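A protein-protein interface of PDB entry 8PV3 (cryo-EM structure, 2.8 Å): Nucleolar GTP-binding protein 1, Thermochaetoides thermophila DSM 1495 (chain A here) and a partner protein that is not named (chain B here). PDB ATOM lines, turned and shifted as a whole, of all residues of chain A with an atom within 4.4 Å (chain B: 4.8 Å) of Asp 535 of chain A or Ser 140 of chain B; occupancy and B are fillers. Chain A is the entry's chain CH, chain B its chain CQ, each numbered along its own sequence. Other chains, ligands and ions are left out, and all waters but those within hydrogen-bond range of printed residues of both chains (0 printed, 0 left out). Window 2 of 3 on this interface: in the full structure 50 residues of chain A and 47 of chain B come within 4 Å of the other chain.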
ATOM      1  N   GLU A 531      19.044 -16.591   7.816  1.00  0.00           N
ATOM      2  CA  GLU A 531      19.848 -16.185   6.670  1.00  0.00           C
ATOM      3  C   GLU A 531      20.405 -14.783   6.864  1.00  0.00           C
ATOM      4  O   GLU A 531      21.557 -14.513   6.515  1.00  0.00           O
ATOM      5  CB  GLU A 531      19.013 -16.261   5.392  1.00  0.00           C
ATOM      6  CG  GLU A 531      19.786 -15.938   4.123  1.00  0.00           C
ATOM      7  CD  GLU A 531      18.941 -16.080   2.872  1.00  0.00           C
ATOM      8  OE1 GLU A 531      17.742 -16.398   3.002  1.00  0.00           O
ATOM      9  OE2 GLU A 531      19.473 -15.877   1.760  1.00  0.00           O
ATOM     10  N   ASP A 532      19.601 -13.882   7.436  1.00  0.00           N
ATOM     11  CA  ASP A 532      20.068 -12.527   7.718  1.00  0.00           C
ATOM     12  C   ASP A 532      21.214 -12.536   8.722  1.00  0.00           C
ATOM     13  O   ASP A 532      22.216 -11.837   8.539  1.00  0.00           O
ATOM     14  CB  ASP A 532      18.907 -11.680   8.235  1.00  0.00           C
ATOM     15  CG  ASP A 532      19.256 -10.210   8.336  1.00  0.00           C
ATOM     16  OD1 ASP A 532      20.212  -9.775   7.661  1.00  0.00           O
ATOM     17  OD2 ASP A 532      18.574  -9.490   9.095  1.00  0.00           O
ATOM     18  N   HIS A 533      21.091 -13.342   9.782  1.00  0.00           N
ATOM     19  CA  HIS A 533      22.143 -13.395  10.794  1.00  0.00           C
ATOM     20  C   HIS A 533      23.428 -13.992  10.227  1.00  0.00           C
ATOM     21  O   HIS A 533      24.525 -13.477  10.475  1.00  0.00           O
ATOM     22  CB  HIS A 533      21.674 -14.195  12.007  1.00  0.00           C
ATOM     23  CG  HIS A 533      22.684 -14.264  13.110  1.00  0.00           C
ATOM     24  ND1 HIS A 533      22.804 -13.284  14.071  1.00  0.00           N
ATOM     25  CD2 HIS A 533      23.629 -15.190  13.396  1.00  0.00           C
ATOM     26  CE1 HIS A 533      23.774 -13.607  14.907  1.00  0.00           C
ATOM     27  NE2 HIS A 533      24.291 -14.760  14.521  1.00  0.00           N
ATOM     28  N   LEU A 534      23.313 -15.075   9.453  1.00  0.00           N
ATOM     29  CA  LEU A 534      24.511 -15.689   8.887  1.00  0.00           C
ATOM     30  C   LEU A 534      25.134 -14.803   7.817  1.00  0.00           C
ATOM     31  O   LEU A 534      26.360 -14.789   7.646  1.00  0.00           O
ATOM     32  CB  LEU A 534      24.192 -17.069   8.315  1.00  0.00           C
ATOM     33  CG  LEU A 534      23.773 -18.123   9.336  1.00  0.00           C
ATOM     34  CD1 LEU A 534      23.355 -19.405   8.633  1.00  0.00           C
ATOM     35  CD2 LEU A 534      24.883 -18.372  10.342  1.00  0.00           C
ATOM     36  N   ASP A 535      24.308 -14.050   7.093  1.00  0.00           N
ATOM     37  CA  ASP A 535      24.818 -13.132   6.086  1.00  0.00           C
ATOM     38  C   ASP A 535      25.548 -11.965   6.738  1.00  0.00           C
ATOM     39  O   ASP A 535      26.571 -11.498   6.226  1.00  0.00           O
ATOM     40  CB  ASP A 535      23.663 -12.661   5.201  1.00  0.00           C
ATOM     41  CG  ASP A 535      24.083 -11.628   4.183  1.00  0.00           C
ATOM     42  OD1 ASP A 535      24.424 -12.015   3.046  1.00  0.00           O
ATOM     43  OD2 ASP A 535      24.030 -10.426   4.503  1.00  0.00           O
ATOM     44  N   GLN A 536      25.043 -11.486   7.880  1.00  0.00           N
ATOM     45  CA  GLN A 536      25.787 -10.496   8.652  1.00  0.00           C
ATOM     46  C   GLN A 536      27.081 -11.063   9.223  1.00  0.00           C
ATOM     47  O   GLN A 536      28.087 -10.347   9.272  1.00  0.00           O
ATOM     48  CB  GLN A 536      24.926  -9.933   9.784  1.00  0.00           C
ATOM     49  CG  GLN A 536      23.744  -9.104   9.320  1.00  0.00           C
ATOM     50  CD  GLN A 536      22.912  -8.585  10.474  1.00  0.00           C
ATOM     51  OE1 GLN A 536      23.177  -8.897  11.635  1.00  0.00           O
ATOM     52  NE2 GLN A 536      21.903  -7.780  10.161  1.00  0.00           N
ATOM     53  N   LEU A 537      27.081 -12.322   9.654  1.00  0.00           N
ATOM     54  CA  LEU A 537      28.304 -12.983  10.092  1.00  0.00           C
ATOM     55  C   LEU A 537      29.275 -13.262   8.952  1.00  0.00           C
ATOM     56  O   LEU A 537      30.450 -13.533   9.212  1.00  0.00           O
ATOM     57  CB  LEU A 537      27.980 -14.296  10.808  1.00  0.00           C
ATOM     58  CG  LEU A 537      27.356 -14.196  12.198  1.00  0.00           C
ATOM     59  CD1 LEU A 537      27.122 -15.583  12.761  1.00  0.00           C
ATOM     60  CD2 LEU A 537      28.251 -13.387  13.118  1.00  0.00           C
ATOM     61  N   GLY A 538      28.815 -13.211   7.705  1.00  0.00           N
ATOM     62  CA  GLY A 538      29.715 -13.365   6.580  1.00  0.00           C
ATOM     63  C   GLY A 538      29.787 -14.760   6.010  1.00  0.00           C
ATOM     64  O   GLY A 538      30.864 -15.197   5.593  1.00  0.00           O
ATOM     65  N   VAL A 539      28.672 -15.476   5.981  1.00  0.00           N
ATOM     66  CA  VAL A 539      28.613 -16.830   5.447  1.00  0.00           C
ATOM     67  C   VAL A 539      27.758 -16.820   4.189  1.00  0.00           C
ATOM     68  O   VAL A 539      26.633 -16.305   4.191  1.00  0.00           O
ATOM     69  CB  VAL A 539      28.057 -17.811   6.496  1.00  0.00           C
ATOM     70  CG1 VAL A 539      27.898 -19.200   5.903  1.00  0.00           C
ATOM     71  CG2 VAL A 539      28.970 -17.853   7.709  1.00  0.00           C
ATOM     72  N   LEU B 137      32.390  -7.810   5.991  1.00  0.00           N
ATOM     73  CA  LEU B 137      31.471  -7.712   4.871  1.00  0.00           C
ATOM     74  C   LEU B 137      30.444  -8.835   4.908  1.00  0.00           C
ATOM     75  O   LEU B 137      30.695  -9.920   5.440  1.00  0.00           O
ATOM     76  CB  LEU B 137      32.233  -7.751   3.550  1.00  0.00           C
ATOM     77  CG  LEU B 137      33.159  -6.554   3.362  1.00  0.00           C
ATOM     78  CD1 LEU B 137      34.221  -6.870   2.338  1.00  0.00           C
ATOM     79  CD2 LEU B 137      32.363  -5.330   2.960  1.00  0.00           C
ATOM     80  N   ARG B 138      29.279  -8.558   4.336  1.00  0.00           N
ATOM     81  CA  ARG B 138      28.238  -9.564   4.216  1.00  0.00           C
ATOM     82  C   ARG B 138      28.614 -10.591   3.155  1.00  0.00           C
ATOM     83  O   ARG B 138      29.437 -10.331   2.275  1.00  0.00           O
ATOM     84  CB  ARG B 138      26.907  -8.905   3.863  1.00  0.00           C
ATOM     85  CG  ARG B 138      26.267  -8.143   5.012  1.00  0.00           C
ATOM     86  CD  ARG B 138      25.096  -7.309   4.518  1.00  0.00           C
ATOM     87  NE  ARG B 138      24.217  -6.884   5.601  1.00  0.00           N
ATOM     88  CZ  ARG B 138      23.120  -7.528   5.974  1.00  0.00           C
ATOM     89  NH1 ARG B 138      22.730  -8.637   5.368  1.00  0.00           N
ATOM     90  NH2 ARG B 138      22.391  -7.043   6.975  1.00  0.00           N
ATOM     91  N   GLY B 139      28.010 -11.778   3.254  1.00  0.00           N
ATOM     92  CA  GLY B 139      28.283 -12.819   2.274  1.00  0.00           C
ATOM     93  C   GLY B 139      27.781 -12.472   0.885  1.00  0.00           C
ATOM     94  O   GLY B 139      28.481 -12.678  -0.112  1.00  0.00           O
ATOM     95  N   SER B 140      26.562 -11.932   0.800  1.00  0.00           N
ATOM     96  CA  SER B 140      26.026 -11.501  -0.487  1.00  0.00           C
ATOM     97  C   SER B 140      26.820 -10.328  -1.048  1.00  0.00           C
ATOM     98  O   SER B 140      27.012 -10.223  -2.266  1.00  0.00           O
ATOM     99  CB  SER B 140      24.549 -11.135  -0.344  1.00  0.00           C
ATOM    100  OG  SER B 140      24.370 -10.114   0.621  1.00  0.00           O
ATOM    101  N   GLU B 141      27.297  -9.439  -0.171  1.00  0.00           N
ATOM    102  CA  GLU B 141      28.158  -8.346  -0.607  1.00  0.00           C
ATOM    103  C   GLU B 141      29.477  -8.870  -1.156  1.00  0.00           C
ATOM    104  O   GLU B 141      29.985  -8.362  -2.158  1.00  0.00           O
ATOM    105  CB  GLU B 141      28.400  -7.370   0.543  1.00  0.00           C
ATOM    106  CG  GLU B 141      27.155  -6.626   0.995  1.00  0.00           C
ATOM    107  CD  GLU B 141      26.624  -5.673  -0.057  1.00  0.00           C
ATOM    108  OE1 GLU B 141      27.434  -5.122  -0.832  1.00  0.00           O
ATOM    109  OE2 GLU B 141      25.392  -5.478  -0.113  1.00  0.00           O
ATOM    110  N   LYS B 142      30.047  -9.894  -0.512  1.00  0.00           N
ATOM    111  CA  LYS B 142      31.273 -10.501  -1.023  1.00  0.00           C
ATOM    112  C   LYS B 142      31.045 -11.161  -2.376  1.00  0.00           C
ATOM    113  O   LYS B 142      31.892 -11.062  -3.269  1.00  0.00           O
ATOM    114  CB  LYS B 142      31.826 -11.517  -0.024  1.00  0.00           C
ATOM    115  CG  LYS B 142      32.476 -10.907   1.204  1.00  0.00           C
ATOM    116  CD  LYS B 142      33.325 -11.937   1.932  1.00  0.00           C
ATOM    117  CE  LYS B 142      33.940 -11.358   3.195  1.00  0.00           C
ATOM    118  NZ  LYS B 142      32.912 -11.093   4.240  1.00  0.00           N
ATOM    119  N   ARG B 143      29.902 -11.835  -2.546  1.00  0.00           N
ATOM    120  CA  ARG B 143      29.582 -12.445  -3.835  1.00  0.00           C
ATOM    121  C   ARG B 143      29.426 -11.394  -4.931  1.00  0.00           C
ATOM    122  O   ARG B 143      29.945 -11.556  -6.046  1.00  0.00           O
ATOM    123  CB  ARG B 143      28.310 -13.287  -3.719  1.00  0.00           C
ATOM    124  CG  ARG B 143      28.443 -14.500  -2.817  1.00  0.00           C
ATOM    125  CD  ARG B 143      29.378 -15.535  -3.418  1.00  0.00           C
ATOM    126  NE  ARG B 143      28.892 -16.022  -4.703  1.00  0.00           N
ATOM    127  CZ  ARG B 143      28.036 -17.024  -4.850  1.00  0.00           C
ATOM    128  NH1 ARG B 143      27.545 -17.672  -3.806  1.00  0.00           N
ATOM    129  NH2 ARG B 143      27.662 -17.385  -6.074  1.00  0.00           N
ATOM    130  N   ARG B 144      28.727 -10.295  -4.628  1.00  0.00           N
ATOM    131  CA  ARG B 144      28.510  -9.275  -5.647  1.00  0.00           C
ATOM    132  C   ARG B 144      29.796  -8.508  -5.946  1.00  0.00           C
ATOM    133  O   ARG B 144      30.035  -8.112  -7.091  1.00  0.00           O
ATOM    134  CB  ARG B 144      27.363  -8.340  -5.238  1.00  0.00           C
ATOM    135  CG  ARG B 144      27.721  -7.150  -4.365  1.00  0.00           C
ATOM    136  CD  ARG B 144      26.694  -6.043  -4.531  1.00  0.00           C
ATOM    137  NE  ARG B 144      27.127  -4.792  -3.921  1.00  0.00           N
ATOM    138  CZ  ARG B 144      26.439  -3.660  -3.969  1.00  0.00           C
ATOM    139  NH1 ARG B 144      25.275  -3.584  -4.593  1.00  0.00           N
ATOM    140  NH2 ARG B 144      26.930  -2.577  -3.376  1.00  0.00           N
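NH2 of Arg 138 of chain B lies within salt-bridge range of OD1 of Asp 532 of chain A, 3.6 Å away.
The side-chain carboxylate (OD2) of Asp 535 of chain A is in salt-bridge range of the guanidinium group (NE) of Arg 138 of chain B (3.7 Å).
NH2 of Arg 138 of chain B sits close to NE2 of Gln 536 of chain A, 3.3 Å away.
The backbone NH (N) of Gly 139 of chain B sits at hydrogen-bond distance from the backbone carbonyl oxygen (O) of Asp 535 of chain A (3.3 Å).
OG of Ser 140 of chain B sits at hydrogen-bond distance from OD1 of Asp 535 of chain A (3.1 Å).
The side-chain amino group (NZ) of Lys 142 of chain B lies within hydrogen-bond range of the backbone carbonyl oxygen (O) of Leu 137 of chain B, at 2.8 Å.
Among the printed residues, merely in contact across the chains: Gly 538 of chain A with Leu 137 of chain B (3.8 Å).
Printed residues of chain B within 4 Å of Asp 535 of chain A: Arg 138 (2.4 Å), Gly 139 (3.3 Å) and Ser 140 (3.1 Å).
Printed residues of chain B within 4 Å of Gln 536 of chain A: Arg 138.
Of the printed residues of chain A, Gly 139 of chain B touches Asp 535 (3.3 Å).
Of the printed residues of chain A, Ser 140 of chain B touches Asp 535 (3.1 Å).
The nearest residue of chain B that does not touch Asp 535 of chain A is Leu 137 of chain B (4.5 Å).
The nearest printed residue of chain A that does not touch Ser 140 of chain B is Val 539 of chain A (5.5 Å).
The nearest printed residue of chain A that does not touch Gly 139 of chain B is Gly 538 of chain A (4.1 Å).
Printed residues of chain A that touch a printed residue of chain B: Asp 532, Asp 535, Gln 536 and Gly 538.
Printed residues of chain B that touch a printed residue of chain A: Leu 137, Arg 138, Gly 139 and Ser 140.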
